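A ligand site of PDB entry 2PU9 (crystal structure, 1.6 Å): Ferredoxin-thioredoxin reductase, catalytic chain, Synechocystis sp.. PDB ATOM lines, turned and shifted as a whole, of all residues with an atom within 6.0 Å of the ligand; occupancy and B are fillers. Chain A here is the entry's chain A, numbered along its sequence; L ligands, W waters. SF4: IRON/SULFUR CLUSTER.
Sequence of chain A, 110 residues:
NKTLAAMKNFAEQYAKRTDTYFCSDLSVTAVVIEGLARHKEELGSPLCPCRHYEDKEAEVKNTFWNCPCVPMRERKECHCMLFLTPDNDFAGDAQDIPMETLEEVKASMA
SG of Cys 69 lies close to N of Met 72 (3.6 Å).
N of Cys 67 is in hydrogen-bond range of O of Pro 46 (2.9 Å).
SG of Cys 78 lies close to N of Phe 83, at 3.4 Å.
The side-chain sulfur (SG) of Cys 78 sits close to the backbone NH (N) of Met 81.
The side-chain sulfur (SG) of Cys 80 lies close to the side-chain sulfur (SG) of Cys 48 (3.1 Å).
The backbone NH (N) of Cys 48 lies within hydrogen-bond range of the backbone carbonyl oxygen (O) of Trp 65, at 2.8 Å.
N of Cys 50 lies close to SG of Cys 48, 3.5 Å away.
N of Met 72 lies within hydrogen-bond range of O of Glu 77 (3.3 Å).
SG of Cys 69 binds FE4 of the ligand, at 2.3 Å.
FE3 of the ligand is bound by SG of Cys 67 (2.3 Å).
SG of Cys 78 binds FE1 of the ligand (2.3 Å).
An iron atom (FE2) of the ligand is bound by the side-chain sulfur (SG) of Cys 48 (2.5 Å).
The backbone NH (N) of Cys 80 sits close to a sulfur (S3) of the ligand, 3.6 Å away.
S4 of the ligand sits close to SG of Cys 80 (3.4 Å).
The backbone NH (N) of His 79 sits close to a sulfur (S3) of the ligand (3.3 Å).
Val 32 touches the ligand (CG1 to S4, 3.8 Å).
Trp 65 touches the ligand (O to S1, 3.98 Å).
Pro 68 touches the ligand (CA to S2, 3.98 Å).
Met 72 touches the ligand (CB to S2, 3.4 Å).
Phe 83 touches the ligand.
The nearest printed residue that does not touch the ligand is Leu 82 (4.03 Å).
Water W2 lies within hydrogen-bond range of O of Glu 77 (2.8 Å), N of His 79 (3.1 Å) and S3 of the ligand (3.3 Å).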
ATOM      1  N   PHE A  10      32.796  17.606 -13.589  1.00  0.00           N
ATOM      2  CA  PHE A  10      31.838  18.715 -13.603  1.00  0.00           C
ATOM      3  C   PHE A  10      32.560  20.004 -13.215  1.00  0.00           C
ATOM      4  O   PHE A  10      32.415  21.034 -13.884  1.00  0.00           O
ATOM      5  CB  PHE A  10      30.700  18.453 -12.600  1.00  0.00           C
ATOM      6  CG  PHE A  10      30.085  19.713 -12.041  1.00  0.00           C
ATOM      7  CD1 PHE A  10      29.290  20.525 -12.838  1.00  0.00           C
ATOM      8  CD2 PHE A  10      30.365  20.107 -10.746  1.00  0.00           C
ATOM      9  CE1 PHE A  10      28.777  21.722 -12.341  1.00  0.00           C
ATOM     10  CE2 PHE A  10      29.854  21.300 -10.236  1.00  0.00           C
ATOM     11  CZ  PHE A  10      29.065  22.115 -11.040  1.00  0.00           C
ATOM     12  N   TYR A  14      32.889  23.202 -15.527  1.00  0.00           N
ATOM     13  CA  TYR A  14      32.183  24.420 -15.118  1.00  0.00           C
ATOM     14  C   TYR A  14      33.157  25.589 -14.971  1.00  0.00           C
ATOM     15  O   TYR A  14      32.824  26.721 -15.299  1.00  0.00           O
ATOM     16  CB  TYR A  14      31.432  24.212 -13.807  1.00  0.00           C
ATOM     17  CG  TYR A  14      30.410  25.293 -13.522  1.00  0.00           C
ATOM     18  CD1 TYR A  14      29.282  25.447 -14.341  1.00  0.00           C
ATOM     19  CD2 TYR A  14      30.583  26.185 -12.471  1.00  0.00           C
ATOM     20  CE1 TYR A  14      28.351  26.460 -14.102  1.00  0.00           C
ATOM     21  CE2 TYR A  14      29.660  27.206 -12.224  1.00  0.00           C
ATOM     22  CZ  TYR A  14      28.554  27.341 -13.046  1.00  0.00           C
ATOM     23  OH  TYR A  14      27.651  28.356 -12.813  1.00  0.00           O
ATOM     24  N   VAL A  32      36.492  20.253  -1.502  1.00  0.00           N
ATOM     25  CA  VAL A  32      35.172  20.717  -1.904  1.00  0.00           C
ATOM     26  C   VAL A  32      34.525  19.727  -2.874  1.00  0.00           C
ATOM     27  O   VAL A  32      33.338  19.451  -2.776  1.00  0.00           O
ATOM     28  CB  VAL A  32      35.230  22.096  -2.575  1.00  0.00           C
ATOM     29  CG1 VAL A  32      33.844  22.470  -3.101  1.00  0.00           C
ATOM     30  CG2 VAL A  32      35.718  23.130  -1.588  1.00  0.00           C
ATOM     31  N   LEU A  36      31.069  17.751  -2.252  1.00  0.00           N
ATOM     32  CA  LEU A  36      29.959  17.808  -3.201  1.00  0.00           C
ATOM     33  C   LEU A  36      29.554  16.375  -3.539  1.00  0.00           C
ATOM     34  O   LEU A  36      28.372  16.030  -3.560  1.00  0.00           O
ATOM     35  CB  LEU A  36      30.393  18.551  -4.476  1.00  0.00           C
ATOM     36  CG  LEU A  36      30.474  20.082  -4.355  1.00  0.00           C
ATOM     37  CD1 LEU A  36      31.203  20.663  -5.552  1.00  0.00           C
ATOM     38  CD2 LEU A  36      29.071  20.661  -4.239  1.00  0.00           C
ATOM     39  N   PRO A  46      24.031  17.667  -5.304  1.00  0.00           N
ATOM     40  CA  PRO A  46      25.264  18.160  -4.688  1.00  0.00           C
ATOM     41  C   PRO A  46      25.111  19.452  -3.887  1.00  0.00           C
ATOM     42  O   PRO A  46      25.548  20.513  -4.333  1.00  0.00           O
ATOM     43  CB  PRO A  46      26.191  18.329  -5.889  1.00  0.00           C
ATOM     44  CG  PRO A  46      25.251  18.753  -6.971  1.00  0.00           C
ATOM     45  CD  PRO A  46      24.071  17.831  -6.769  1.00  0.00           C
ATOM     46  N   LEU A  47      24.504  19.371  -2.713  1.00  0.00           N
ATOM     47  CA  LEU A  47      24.348  20.545  -1.864  1.00  0.00           C
ATOM     48  C   LEU A  47      25.740  21.066  -1.506  1.00  0.00           C
ATOM     49  O   LEU A  47      26.667  20.282  -1.286  1.00  0.00           O
ATOM     50  CB  LEU A  47      23.611  20.207  -0.571  1.00  0.00           C
ATOM     51  CG  LEU A  47      22.091  20.087  -0.567  1.00  0.00           C
ATOM     52  CD1 LEU A  47      21.619  19.783   0.844  1.00  0.00           C
ATOM     53  CD2 LEU A  47      21.468  21.386  -1.055  1.00  0.00           C
ATOM     54  N   CYS A  48      25.876  22.379  -1.453  1.00  0.00           N
ATOM     55  CA  CYS A  48      27.149  22.986  -1.112  1.00  0.00           C
ATOM     56  C   CYS A  48      27.704  22.403   0.193  1.00  0.00           C
ATOM     57  O   CYS A  48      26.978  22.299   1.190  1.00  0.00           O
ATOM     58  CB  CYS A  48      26.964  24.500  -0.954  1.00  0.00           C
ATOM     59  SG  CYS A  48      28.503  25.338  -0.633  1.00  0.00           S
ATOM     60  N   PRO A  49      28.992  22.015   0.195  1.00  0.00           N
ATOM     61  CA  PRO A  49      29.581  21.448   1.416  1.00  0.00           C
ATOM     62  C   PRO A  49      30.102  22.476   2.423  1.00  0.00           C
ATOM     63  O   PRO A  49      30.600  22.102   3.478  1.00  0.00           O
ATOM     64  CB  PRO A  49      30.700  20.565   0.858  1.00  0.00           C
ATOM     65  CG  PRO A  49      31.204  21.384  -0.281  1.00  0.00           C
ATOM     66  CD  PRO A  49      29.913  21.855  -0.951  1.00  0.00           C
ATOM     67  N   CYS A  50      29.973  23.759   2.096  1.00  0.00           N
ATOM     68  CA  CYS A  50      30.447  24.823   2.981  1.00  0.00           C
ATOM     69  C   CYS A  50      29.304  25.612   3.606  1.00  0.00           C
ATOM     70  O   CYS A  50      29.465  26.784   3.959  1.00  0.00           O
ATOM     71  CB  CYS A  50      31.391  25.765   2.234  1.00  0.00           C
ATOM     72  SG  CYS A  50      32.882  24.934   1.635  1.00  0.00           S
ATOM     73  N   TRP A  65      21.025  25.993  -2.730  1.00  0.00           N
ATOM     74  CA  TRP A  65      22.391  25.566  -2.485  1.00  0.00           C
ATOM     75  C   TRP A  65      22.873  24.351  -3.273  1.00  0.00           C
ATOM     76  O   TRP A  65      23.923  23.793  -2.961  1.00  0.00           O
ATOM     77  CB  TRP A  65      22.589  25.323  -0.981  1.00  0.00           C
ATOM     78  CG  TRP A  65      22.556  26.594  -0.167  1.00  0.00           C
ATOM     79  CD1 TRP A  65      21.693  26.898   0.850  1.00  0.00           C
ATOM     80  CD2 TRP A  65      23.440  27.724  -0.283  1.00  0.00           C
ATOM     81  NE1 TRP A  65      21.975  28.138   1.370  1.00  0.00           N
ATOM     82  CE2 TRP A  65      23.043  28.670   0.680  1.00  0.00           C
ATOM     83  CE3 TRP A  65      24.519  28.020  -1.127  1.00  0.00           C
ATOM     84  CZ2 TRP A  65      23.697  29.901   0.838  1.00  0.00           C
ATOM     85  CZ3 TRP A  65      25.160  29.240  -0.968  1.00  0.00           C
ATOM     86  CH2 TRP A  65      24.751  30.163   0.005  1.00  0.00           C
ATOM     87  N   ASN A  66      22.104  23.927  -4.262  1.00  0.00           N
ATOM     88  CA  ASN A  66      22.542  22.805  -5.089  1.00  0.00           C
ATOM     89  C   ASN A  66      23.609  23.361  -6.035  1.00  0.00           C
ATOM     90  O   ASN A  66      23.366  24.321  -6.756  1.00  0.00           O
ATOM     91  CB  ASN A  66      21.367  22.194  -5.865  1.00  0.00           C
ATOM     92  CG  ASN A  66      20.485  21.301  -4.997  1.00  0.00           C
ATOM     93  OD1 ASN A  66      20.916  20.806  -3.963  1.00  0.00           O
ATOM     94  ND2 ASN A  66      19.242  21.088  -5.432  1.00  0.00           N
ATOM     95  N   CYS A  67      24.794  22.759  -6.021  1.00  0.00           N
ATOM     96  CA  CYS A  67      25.905  23.210  -6.856  1.00  0.00           C
ATOM     97  C   CYS A  67      25.693  22.995  -8.363  1.00  0.00           C
ATOM     98  O   CYS A  67      25.353  21.903  -8.788  1.00  0.00           O
ATOM     99  CB  CYS A  67      27.186  22.515  -6.416  1.00  0.00           C
ATOM    100  SG  CYS A  67      28.699  23.228  -7.118  1.00  0.00           S
ATOM    101  N   PRO A  68      25.909  24.045  -9.178  1.00  0.00           N
ATOM    102  CA  PRO A  68      26.329  25.391  -8.793  1.00  0.00           C
ATOM    103  C   PRO A  68      25.173  26.169  -8.168  1.00  0.00           C
ATOM    104  O   PRO A  68      24.092  26.277  -8.755  1.00  0.00           O
ATOM    105  CB  PRO A  68      26.825  26.000 -10.104  1.00  0.00           C
ATOM    106  CG  PRO A  68      25.940  25.342 -11.122  1.00  0.00           C
ATOM    107  CD  PRO A  68      25.864  23.905 -10.645  1.00  0.00           C
ATOM    108  N   CYS A  69      25.415  26.700  -6.982  1.00  0.00           N
ATOM    109  CA  CYS A  69      24.400  27.445  -6.232  1.00  0.00           C
ATOM    110  C   CYS A  69      23.980  28.760  -6.864  1.00  0.00           C
ATOM    111  O   CYS A  69      24.589  29.246  -7.822  1.00  0.00           O
ATOM    112  CB  CYS A  69      24.917  27.724  -4.810  1.00  0.00           C
ATOM    113  SG  CYS A  69      26.439  28.701  -4.783  1.00  0.00           S
ATOM    114  N   VAL A  70      22.917  29.346  -6.322  1.00  0.00           N
ATOM    115  CA  VAL A  70      22.425  30.609  -6.856  1.00  0.00           C
ATOM    116  C   VAL A  70      23.490  31.712  -6.831  1.00  0.00           C
ATOM    117  O   VAL A  70      23.655  32.427  -7.823  1.00  0.00           O
ATOM    118  CB  VAL A  70      21.163  31.053  -6.096  1.00  0.00           C
ATOM    119  CG1 VAL A  70      20.852  32.520  -6.354  1.00  0.00           C
ATOM    120  CG2 VAL A  70      19.984  30.206  -6.534  1.00  0.00           C
ATOM    121  N   PRO A  71      24.226  31.866  -5.710  1.00  0.00           N
ATOM    122  CA  PRO A  71      25.250  32.917  -5.690  1.00  0.00           C
ATOM    123  C   PRO A  71      26.271  32.751  -6.807  1.00  0.00           C
ATOM    124  O   PRO A  71      26.737  33.739  -7.393  1.00  0.00           O
ATOM    125  CB  PRO A  71      25.865  32.762  -4.311  1.00  0.00           C
ATOM    126  CG  PRO A  71      24.674  32.384  -3.482  1.00  0.00           C
ATOM    127  CD  PRO A  71      23.992  31.343  -4.353  1.00  0.00           C
ATOM    128  N   MET A  72      26.630  31.504  -7.112  1.00  0.00           N
ATOM    129  CA  MET A  72      27.589  31.237  -8.177  1.00  0.00           C
ATOM    130  C   MET A  72      26.964  31.460  -9.542  1.00  0.00           C
ATOM    131  O   MET A  72      27.526  32.173 -10.387  1.00  0.00           O
ATOM    132  CB  MET A  72      28.105  29.802  -8.082  1.00  0.00           C
ATOM    133  CG  MET A  72      29.119  29.447  -9.162  1.00  0.00           C
ATOM    134  SD  MET A  72      30.616  30.456  -9.105  1.00  0.00           S
ATOM    135  CE  MET A  72      31.245  30.190 -10.761  1.00  0.00           C
ATOM    136  N   GLU A  77      29.894  33.990  -7.394  1.00  0.00           N
ATOM    137  CA  GLU A  77      30.466  34.003  -6.054  1.00  0.00           C
ATOM    138  C   GLU A  77      30.382  32.585  -5.502  1.00  0.00           C
ATOM    139  O   GLU A  77      29.292  32.061  -5.264  1.00  0.00           O
ATOM    140  CB  GLU A  77      29.688  34.968  -5.147  1.00  0.00           C
ATOM    141  CG  GLU A  77      29.894  36.425  -5.541  1.00  0.00           C
ATOM    142  CD  GLU A  77      29.069  37.385  -4.694  1.00  0.00           C
ATOM    143  OE1 GLU A  77      28.390  36.923  -3.751  1.00  0.00           O
ATOM    144  OE2 GLU A  77      29.110  38.600  -4.987  1.00  0.00           O
ATOM    145  N   CYS A  78      31.555  31.975  -5.322  1.00  0.00           N
ATOM    146  CA  CYS A  78      31.664  30.611  -4.795  1.00  0.00           C
ATOM    147  C   CYS A  78      32.360  30.652  -3.436  1.00  0.00           C
ATOM    148  O   CYS A  78      33.590  30.739  -3.351  1.00  0.00           O
ATOM    149  CB  CYS A  78      32.470  29.742  -5.778  1.00  0.00           C
ATOM    150  SG  CYS A  78      32.794  28.047  -5.206  1.00  0.00           S
ATOM    151  N   HIS A  79      31.572  30.598  -2.366  1.00  0.00           N
ATOM    152  CA  HIS A  79      32.094  30.637  -1.015  1.00  0.00           C
ATOM    153  C   HIS A  79      33.047  29.473  -0.708  1.00  0.00           C
ATOM    154  O   HIS A  79      33.963  29.618   0.108  1.00  0.00           O
ATOM    155  CB  HIS A  79      30.928  30.617  -0.019  1.00  0.00           C
ATOM    156  CG  HIS A  79      31.347  30.373   1.399  1.00  0.00           C
ATOM    157  ND1 HIS A  79      32.156  31.237   2.102  1.00  0.00           N
ATOM    158  CD2 HIS A  79      31.079  29.343   2.247  1.00  0.00           C
ATOM    159  CE1 HIS A  79      32.374  30.760   3.307  1.00  0.00           C
ATOM    160  NE2 HIS A  79      31.737  29.605   3.423  1.00  0.00           N
ATOM    161  N   CYS A  80      32.835  28.333  -1.349  1.00  0.00           N
ATOM    162  CA  CYS A  80      33.677  27.162  -1.134  1.00  0.00           C
ATOM    163  C   CYS A  80      35.086  27.322  -1.667  1.00  0.00           C
ATOM    164  O   CYS A  80      35.954  26.510  -1.360  1.00  0.00           O
ATOM    165  CB  CYS A  80      33.066  25.915  -1.795  1.00  0.00           C
ATOM    166  SG  CYS A  80      31.573  25.315  -1.019  1.00  0.00           S
ATOM    167  N   MET A  81      35.300  28.356  -2.464  1.00  0.00           N
ATOM    168  CA  MET A  81      36.598  28.611  -3.081  1.00  0.00           C
ATOM    169  C   MET A  81      36.927  27.539  -4.118  1.00  0.00           C
ATOM    170  O   MET A  81      38.086  27.217  -4.347  1.00  0.00           O
ATOM    171  CB  MET A  81      37.691  28.676  -2.017  1.00  0.00           C
ATOM    172  CG  MET A  81      37.620  29.920  -1.151  1.00  0.00           C
ATOM    173  SD  MET A  81      38.770  29.877   0.245  1.00  0.00           S
ATOM    174  CE  MET A  81      40.342  30.088  -0.587  1.00  0.00           C
ATOM    175  N   LEU A  82      35.886  26.988  -4.733  1.00  0.00           N
ATOM    176  CA  LEU A  82      36.063  25.977  -5.780  1.00  0.00           C
ATOM    177  C   LEU A  82      36.226  26.702  -7.122  1.00  0.00           C
ATOM    178  O   LEU A  82      37.173  26.454  -7.863  1.00  0.00           O
ATOM    179  CB  LEU A  82      34.865  25.018  -5.841  1.00  0.00           C
ATOM    180  CG  LEU A  82      34.845  24.027  -7.005  1.00  0.00           C
ATOM    181  CD1 LEU A  82      36.164  23.265  -7.073  1.00  0.00           C
ATOM    182  CD2 LEU A  82      33.685  23.051  -6.831  1.00  0.00           C
ATOM    183  N   PHE A  83      35.304  27.612  -7.411  1.00  0.00           N
ATOM    184  CA  PHE A  83      35.337  28.387  -8.651  1.00  0.00           C
ATOM    185  C   PHE A  83      35.703  29.822  -8.289  1.00  0.00           C
ATOM    186  O   PHE A  83      34.841  30.624  -7.930  1.00  0.00           O
ATOM    187  CB  PHE A  83      33.974  28.361  -9.337  1.00  0.00           C
ATOM    188  CG  PHE A  83      33.429  26.983  -9.555  1.00  0.00           C
ATOM    189  CD1 PHE A  83      32.281  26.563  -8.897  1.00  0.00           C
ATOM    190  CD2 PHE A  83      34.080  26.094 -10.412  1.00  0.00           C
ATOM    191  CE1 PHE A  83      31.784  25.273  -9.092  1.00  0.00           C
ATOM    192  CE2 PHE A  83      33.597  24.806 -10.609  1.00  0.00           C
ATOM    193  CZ  PHE A  83      32.443  24.393  -9.941  1.00  0.00           C
HETATM  194 FE1  SF4 L   1      30.766  26.949  -4.866  1.00  0.00          FE
HETATM  195 FE2  SF4 L   1      29.467  25.677  -2.861  1.00  0.00          FE
HETATM  196 FE3  SF4 L   1      29.169  24.902  -5.618  1.00  0.00          FE
HETATM  197 FE4  SF4 L   1      28.151  27.227  -4.639  1.00  0.00          FE
HETATM  198  S1  SF4 L   1      27.519  25.131  -4.025  1.00  0.00           S
HETATM  199  S2  SF4 L   1      29.276  26.955  -6.621  1.00  0.00           S
HETATM  200  S3  SF4 L   1      29.709  27.945  -3.101  1.00  0.00           S
HETATM  201  S4  SF4 L   1      31.049  24.754  -4.304  1.00  0.00           S
HETATM  202  O   HOH W   1      28.573  28.537   0.089  1.00  0.00           O
HETATM  203  O   HOH W   2      28.552  31.039  -2.756  1.00  0.00           O
